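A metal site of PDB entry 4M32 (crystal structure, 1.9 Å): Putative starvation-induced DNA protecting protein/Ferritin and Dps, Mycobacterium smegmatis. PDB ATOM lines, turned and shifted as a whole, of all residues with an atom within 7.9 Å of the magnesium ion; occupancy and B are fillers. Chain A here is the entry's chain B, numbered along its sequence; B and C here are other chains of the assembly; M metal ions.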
ATOM      1  N   SER A  54      11.554 -14.554 -15.659  1.00  0.00           N
ATOM      2  CA  SER A  54      10.637 -13.607 -15.018  1.00  0.00           C
ATOM      3  C   SER A  54      11.370 -12.362 -14.518  1.00  0.00           C
ATOM      4  O   SER A  54      12.367 -12.458 -13.791  1.00  0.00           O
ATOM      5  CB  SER A  54       9.884 -14.291 -13.872  1.00  0.00           C
ATOM      6  OG  SER A  54       9.217 -15.446 -14.346  1.00  0.00           O
ATOM      7  N   ASN A  55      10.867 -11.193 -14.922  1.00  0.00           N
ATOM      8  CA  ASN A  55      11.469  -9.883 -14.626  1.00  0.00           C
ATOM      9  C   ASN A  55      12.830  -9.670 -15.319  1.00  0.00           C
ATOM     10  O   ASN A  55      13.734  -9.017 -14.774  1.00  0.00           O
ATOM     11  CB  ASN A  55      11.539  -9.580 -13.121  1.00  0.00           C
ATOM     12  CG  ASN A  55      11.581  -8.100 -12.832  1.00  0.00           C
ATOM     13  OD1 ASN A  55      11.143  -7.285 -13.648  1.00  0.00           O
ATOM     14  ND2 ASN A  55      12.096  -7.731 -11.677  1.00  0.00           N
ATOM     15  N   PHE A  56      12.945 -10.223 -16.523  1.00  0.00           N
ATOM     16  CA  PHE A  56      14.135 -10.068 -17.365  1.00  0.00           C
ATOM     17  C   PHE A  56      14.568  -8.613 -17.494  1.00  0.00           C
ATOM     18  O   PHE A  56      15.741  -8.293 -17.279  1.00  0.00           O
ATOM     19  CB  PHE A  56      13.878 -10.638 -18.769  1.00  0.00           C
ATOM     20  CG  PHE A  56      14.822 -10.109 -19.819  1.00  0.00           C
ATOM     21  CD1 PHE A  56      16.126 -10.585 -19.901  1.00  0.00           C
ATOM     22  CD2 PHE A  56      14.404  -9.128 -20.708  1.00  0.00           C
ATOM     23  CE1 PHE A  56      17.005 -10.091 -20.855  1.00  0.00           C
ATOM     24  CE2 PHE A  56      15.274  -8.620 -21.663  1.00  0.00           C
ATOM     25  CZ  PHE A  56      16.578  -9.096 -21.745  1.00  0.00           C
ATOM     26  N   ARG A  57      13.627  -7.751 -17.849  1.00  0.00           N
ATOM     27  CA  ARG A  57      13.945  -6.374 -18.246  1.00  0.00           C
ATOM     28  C   ARG A  57      14.577  -5.567 -17.114  1.00  0.00           C
ATOM     29  O   ARG A  57      15.608  -4.915 -17.322  1.00  0.00           O
ATOM     30  CB  ARG A  57      12.715  -5.675 -18.829  1.00  0.00           C
ATOM     31  CG  ARG A  57      13.018  -4.317 -19.433  1.00  0.00           C
ATOM     32  CD  ARG A  57      11.798  -3.725 -20.115  1.00  0.00           C
ATOM     33  NE  ARG A  57      12.073  -2.395 -20.648  1.00  0.00           N
ATOM     34  CZ  ARG A  57      11.993  -1.269 -19.960  1.00  0.00           C
ATOM     35  NH1 ARG A  57      11.639  -1.286 -18.672  1.00  0.00           N
ATOM     36  NH2 ARG A  57      12.271  -0.109 -20.550  1.00  0.00           N
ATOM     37  N   ASP A  58      13.984  -5.614 -15.921  1.00  0.00           N
ATOM     38  CA  ASP A  58      14.531  -4.919 -14.756  1.00  0.00           C
ATOM     39  C   ASP A  58      15.980  -5.309 -14.482  1.00  0.00           C
ATOM     40  O   ASP A  58      16.833  -4.439 -14.269  1.00  0.00           O
ATOM     41  CB  ASP A  58      13.695  -5.181 -13.502  1.00  0.00           C
ATOM     42  CG  ASP A  58      12.642  -4.108 -13.267  1.00  0.00           C
ATOM     43  OD1 ASP A  58      12.907  -2.919 -13.542  1.00  0.00           O
ATOM     44  OD2 ASP A  58      11.555  -4.461 -12.773  1.00  0.00           O
ATOM     45  N   LEU A  59      16.259  -6.617 -14.494  1.00  0.00           N
ATOM     46  CA  LEU A  59      17.604  -7.112 -14.228  1.00  0.00           C
ATOM     47  C   LEU A  59      18.576  -6.725 -15.330  1.00  0.00           C
ATOM     48  O   LEU A  59      19.686  -6.257 -15.040  1.00  0.00           O
ATOM     49  CB  LEU A  59      17.603  -8.636 -14.016  1.00  0.00           C
ATOM     50  CG  LEU A  59      17.584  -9.172 -12.572  1.00  0.00           C
ATOM     51  CD1 LEU A  59      18.834  -8.736 -11.799  1.00  0.00           C
ATOM     52  CD2 LEU A  59      16.301  -8.752 -11.834  1.00  0.00           C
ATOM     53  N   GLU A 164      15.268  -8.425  -5.282  1.00  0.00           N
ATOM     54  CA  GLU A 164      14.414  -9.227  -6.157  1.00  0.00           C
ATOM     55  C   GLU A 164      14.103 -10.618  -5.575  1.00  0.00           C
ATOM     56  O   GLU A 164      12.984 -11.117  -5.702  1.00  0.00           O
ATOM     57  CB  GLU A 164      15.050  -9.361  -7.555  1.00  0.00           C
ATOM     58  CG  GLU A 164      14.356 -10.333  -8.522  1.00  0.00           C
ATOM     59  CD  GLU A 164      12.983  -9.846  -9.009  1.00  0.00           C
ATOM     60  OE1 GLU A 164      12.158 -10.714  -9.384  1.00  0.00           O
ATOM     61  OE2 GLU A 164      12.733  -8.630  -9.016  1.00  0.00           O
ATOM     62  N   SER B  54       9.641 -10.072  -5.607  1.00  0.00           N
ATOM     63  CA  SER B  54       9.468 -10.170  -7.055  1.00  0.00           C
ATOM     64  C   SER B  54       9.040  -8.858  -7.703  1.00  0.00           C
ATOM     65  O   SER B  54       8.065  -8.236  -7.289  1.00  0.00           O
ATOM     66  CB  SER B  54       8.454 -11.268  -7.400  1.00  0.00           C
ATOM     67  OG  SER B  54       8.925 -12.524  -6.964  1.00  0.00           O
ATOM     68  N   ASN B  55       9.781  -8.467  -8.731  1.00  0.00           N
ATOM     69  CA  ASN B  55       9.604  -7.192  -9.430  1.00  0.00           C
ATOM     70  C   ASN B  55       9.871  -5.965  -8.554  1.00  0.00           C
ATOM     71  O   ASN B  55       9.225  -4.911  -8.711  1.00  0.00           O
ATOM     72  CB  ASN B  55       8.226  -7.099 -10.113  1.00  0.00           C
ATOM     73  CG  ASN B  55       8.246  -6.148 -11.297  1.00  0.00           C
ATOM     74  OD1 ASN B  55       9.296  -5.932 -11.905  1.00  0.00           O
ATOM     75  ND2 ASN B  55       7.098  -5.583 -11.629  1.00  0.00           N
ATOM     76  N   PHE B  56      10.840  -6.109  -7.649  1.00  0.00           N
ATOM     77  CA  PHE B  56      11.279  -5.033  -6.768  1.00  0.00           C
ATOM     78  C   PHE B  56      11.551  -3.743  -7.536  1.00  0.00           C
ATOM     79  O   PHE B  56      11.023  -2.694  -7.188  1.00  0.00           O
ATOM     80  CB  PHE B  56      12.544  -5.450  -5.997  1.00  0.00           C
ATOM     81  CG  PHE B  56      13.324  -4.282  -5.433  1.00  0.00           C
ATOM     82  CD1 PHE B  56      14.437  -3.779  -6.110  1.00  0.00           C
ATOM     83  CD2 PHE B  56      12.931  -3.670  -4.257  1.00  0.00           C
ATOM     84  CE1 PHE B  56      15.154  -2.701  -5.611  1.00  0.00           C
ATOM     85  CE2 PHE B  56      13.642  -2.574  -3.746  1.00  0.00           C
ATOM     86  CZ  PHE B  56      14.753  -2.094  -4.425  1.00  0.00           C
ATOM     87  N   ARG B  57      12.390  -3.842  -8.573  1.00  0.00           N
ATOM     88  CA  ARG B  57      12.910  -2.646  -9.247  1.00  0.00           C
ATOM     89  C   ARG B  57      11.812  -1.778  -9.856  1.00  0.00           C
ATOM     90  O   ARG B  57      11.800  -0.567  -9.658  1.00  0.00           O
ATOM     91  CB  ARG B  57      13.967  -3.018 -10.297  1.00  0.00           C
ATOM     92  CG  ARG B  57      14.714  -1.819 -10.869  1.00  0.00           C
ATOM     93  CD  ARG B  57      15.803  -2.250 -11.841  1.00  0.00           C
ATOM     94  NE  ARG B  57      16.459  -1.110 -12.476  1.00  0.00           N
ATOM     95  CZ  ARG B  57      16.040  -0.515 -13.594  1.00  0.00           C
ATOM     96  NH1 ARG B  57      14.954  -0.952 -14.221  1.00  0.00           N
ATOM     97  NH2 ARG B  57      16.716   0.515 -14.088  1.00  0.00           N
ATOM     98  N   ASP B  58      10.883  -2.402 -10.585  1.00  0.00           N
ATOM     99  CA  ASP B  58       9.754  -1.682 -11.181  1.00  0.00           C
ATOM    100  C   ASP B  58       8.959  -0.904 -10.136  1.00  0.00           C
ATOM    101  O   ASP B  58       8.629   0.260 -10.351  1.00  0.00           O
ATOM    102  CB  ASP B  58       8.813  -2.639 -11.917  1.00  0.00           C
ATOM    103  CG  ASP B  58       9.107  -2.723 -13.400  1.00  0.00           C
ATOM    104  OD1 ASP B  58       9.548  -1.729 -14.018  1.00  0.00           O
ATOM    105  OD2 ASP B  58       8.866  -3.817 -13.969  1.00  0.00           O
ATOM    106  N   LEU B  59       8.657  -1.563  -9.003  1.00  0.00           N
ATOM    107  CA  LEU B  59       7.909  -0.936  -7.911  1.00  0.00           C
ATOM    108  C   LEU B  59       8.699   0.176  -7.228  1.00  0.00           C
ATOM    109  O   LEU B  59       8.166   1.264  -7.013  1.00  0.00           O
ATOM    110  CB  LEU B  59       7.438  -1.976  -6.879  1.00  0.00           C
ATOM    111  CG  LEU B  59       5.990  -2.446  -6.973  1.00  0.00           C
ATOM    112  CD1 LEU B  59       5.026  -1.251  -6.900  1.00  0.00           C
ATOM    113  CD2 LEU B  59       5.750  -3.269  -8.236  1.00  0.00           C
ATOM    114  N   GLU B 164       0.146  -4.567 -11.357  1.00  0.00           N
ATOM    115  CA  GLU B 164       1.083  -5.634 -10.983  1.00  0.00           C
ATOM    116  C   GLU B 164       0.388  -6.845 -10.354  1.00  0.00           C
ATOM    117  O   GLU B 164       0.760  -7.994 -10.625  1.00  0.00           O
ATOM    118  CB  GLU B 164       2.157  -5.080 -10.030  1.00  0.00           C
ATOM    119  CG  GLU B 164       3.070  -6.134  -9.387  1.00  0.00           C
ATOM    120  CD  GLU B 164       3.986  -6.861 -10.366  1.00  0.00           C
ATOM    121  OE1 GLU B 164       4.363  -6.267 -11.408  1.00  0.00           O
ATOM    122  OE2 GLU B 164       4.337  -8.029 -10.097  1.00  0.00           O
ATOM    123  N   SER C  54       1.765  -9.775 -13.392  1.00  0.00           N
ATOM    124  CA  SER C  54       3.152  -9.820 -12.934  1.00  0.00           C
ATOM    125  C   SER C  54       4.123  -9.205 -13.940  1.00  0.00           C
ATOM    126  O   SER C  54       4.117  -9.580 -15.114  1.00  0.00           O
ATOM    127  CB  SER C  54       3.563 -11.261 -12.604  1.00  0.00           C
ATOM    128  OG  SER C  54       2.648 -11.847 -11.683  1.00  0.00           O
ATOM    129  N   ASN C  55       4.925  -8.265 -13.464  1.00  0.00           N
ATOM    130  CA  ASN C  55       5.867  -7.489 -14.294  1.00  0.00           C
ATOM    131  C   ASN C  55       5.199  -6.610 -15.350  1.00  0.00           C
ATOM    132  O   ASN C  55       5.708  -6.441 -16.459  1.00  0.00           O
ATOM    133  CB  ASN C  55       6.969  -8.374 -14.909  1.00  0.00           C
ATOM    134  CG  ASN C  55       8.231  -7.604 -15.192  1.00  0.00           C
ATOM    135  OD1 ASN C  55       8.504  -6.601 -14.532  1.00  0.00           O
ATOM    136  ND2 ASN C  55       9.009  -8.056 -16.169  1.00  0.00           N
ATOM    137  N   PHE C  56       4.044  -6.047 -14.987  1.00  0.00           N
ATOM    138  CA  PHE C  56       3.302  -5.116 -15.837  1.00  0.00           C
ATOM    139  C   PHE C  56       4.160  -3.954 -16.353  1.00  0.00           C
ATOM    140  O   PHE C  56       4.176  -3.686 -17.553  1.00  0.00           O
ATOM    141  CB  PHE C  56       2.077  -4.549 -15.081  1.00  0.00           C
ATOM    142  CG  PHE C  56       1.603  -3.219 -15.612  1.00  0.00           C
ATOM    143  CD1 PHE C  56       0.792  -3.166 -16.750  1.00  0.00           C
ATOM    144  CD2 PHE C  56       1.967  -2.033 -14.986  1.00  0.00           C
ATOM    145  CE1 PHE C  56       0.356  -1.939 -17.247  1.00  0.00           C
ATOM    146  CE2 PHE C  56       1.541  -0.807 -15.486  1.00  0.00           C
ATOM    147  CZ  PHE C  56       0.731  -0.759 -16.615  1.00  0.00           C
ATOM    148  N   ARG C  57       4.848  -3.279 -15.431  1.00  0.00           N
ATOM    149  CA  ARG C  57       5.522  -2.025 -15.745  1.00  0.00           C
ATOM    150  C   ARG C  57       6.592  -2.206 -16.813  1.00  0.00           C
ATOM    151  O   ARG C  57       6.644  -1.435 -17.770  1.00  0.00           O
ATOM    152  CB  ARG C  57       6.095  -1.390 -14.478  1.00  0.00           C
ATOM    153  CG  ARG C  57       6.538   0.056 -14.651  1.00  0.00           C
ATOM    154  CD  ARG C  57       7.110   0.596 -13.351  1.00  0.00           C
ATOM    155  NE  ARG C  57       7.706   1.926 -13.530  1.00  0.00           N
ATOM    156  CZ  ARG C  57       8.968   2.150 -13.870  1.00  0.00           C
ATOM    157  NH1 ARG C  57       9.809   1.138 -14.068  1.00  0.00           N
ATOM    158  NH2 ARG C  57       9.401   3.389 -14.001  1.00  0.00           N
ATOM    159  N   ASP C  58       7.438  -3.224 -16.649  1.00  0.00           N
ATOM    160  CA  ASP C  58       8.485  -3.531 -17.627  1.00  0.00           C
ATOM    161  C   ASP C  58       7.924  -3.731 -19.025  1.00  0.00           C
ATOM    162  O   ASP C  58       8.464  -3.196 -19.997  1.00  0.00           O
ATOM    163  CB  ASP C  58       9.292  -4.764 -17.214  1.00  0.00           C
ATOM    164  CG  ASP C  58      10.560  -4.426 -16.463  1.00  0.00           C
ATOM    165  OD1 ASP C  58      11.183  -3.370 -16.735  1.00  0.00           O
ATOM    166  OD2 ASP C  58      10.948  -5.229 -15.593  1.00  0.00           O
ATOM    167  N   LEU C  59       6.845  -4.504 -19.138  1.00  0.00           N
ATOM    168  CA  LEU C  59       6.217  -4.766 -20.434  1.00  0.00           C
ATOM    169  C   LEU C  59       5.557  -3.511 -20.989  1.00  0.00           C
ATOM    170  O   LEU C  59       5.737  -3.187 -22.163  1.00  0.00           O
ATOM    171  CB  LEU C  59       5.241  -5.948 -20.367  1.00  0.00           C
ATOM    172  CG  LEU C  59       5.815  -7.311 -20.753  1.00  0.00           C
ATOM    173  CD1 LEU C  59       6.261  -7.328 -22.225  1.00  0.00           C
ATOM    174  CD2 LEU C  59       6.975  -7.745 -19.844  1.00  0.00           C
ATOM    175  N   GLU C 164      11.184 -12.533 -21.123  1.00  0.00           N
ATOM    176  CA  GLU C 164      10.333 -12.590 -19.934  1.00  0.00           C
ATOM    177  C   GLU C 164       9.744 -13.987 -19.693  1.00  0.00           C
ATOM    178  O   GLU C 164       9.659 -14.436 -18.546  1.00  0.00           O
ATOM    179  CB  GLU C 164       9.202 -11.549 -20.052  1.00  0.00           C
ATOM    180  CG  GLU C 164       8.077 -11.661 -19.019  1.00  0.00           C
ATOM    181  CD  GLU C 164       8.504 -11.318 -17.589  1.00  0.00           C
ATOM    182  OE1 GLU C 164       7.838 -11.803 -16.648  1.00  0.00           O
ATOM    183  OE2 GLU C 164       9.492 -10.584 -17.403  1.00  0.00           O
HETATM  184 MG    MG M   1      10.024  -5.528 -13.729  1.00  0.00          MG
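The magnesium ion is bound by OD1 of Asn 55 of chain B (2.0 Å), OD1 of Asn 55 of chain C (2.0 Å), OD2 of Asp 58 of chain B (2.1 Å), OD1 of Asn 55 of chain A (2.1 Å), OD2 of Asp 58 of chain A (2.1 Å) and OD2 of Asp 58 of chain C (2.1 Å).
ND2 of Asn 55 of chain B is in hydrogen-bond range of OE1 of Glu 164 of chain B, at 2.8 Å. The backbone NH (N) of Asn 55 of chain B sits at hydrogen-bond distance from the side-chain carboxylate (OE2) of Glu 164 of chain A (3.0 Å). The side-chain carboxylate (OE1) of Glu 164 of chain B sits at hydrogen-bond distance from the backbone NH (N) of Asn 55 of chain C, 2.9 Å away. The side-chain carboxylate (OD1) of Asp 58 of chain B lies within salt-bridge range of the guanidinium group (NH1) of Arg 57 of chain C. ND2 of Asn 55 of chain A sits at hydrogen-bond distance from OE2 of Glu 164 of chain A, at 2.9 Å. The side-chain carboxylate of Glu 164 of chain C sits at hydrogen-bond distance from the backbone NH of Asn 55 of chain A, 2.9 Å away. The guanidinium group (NH1) of Arg 57 of chain B is in salt-bridge range of the side-chain carboxylate (OD1) of Asp 58 of chain A (2.9 Å). The side-chain carboxylate of Asp 58 of chain C lies within salt-bridge range of the guanidinium group of Arg 57 of chain A, 2.9 Å away.
Six residues have an atom within 4 Å of the magnesium ion: Asn 55 of chain A, Asp 58 of chain A, Asn 55 of chain B, Asp 58 of chain B, Asn 55 of chain C and Asp 58 of chain C. The nearest printed residue that does not touch the magnesium ion is Arg 57 of chain A (5.7 Å).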
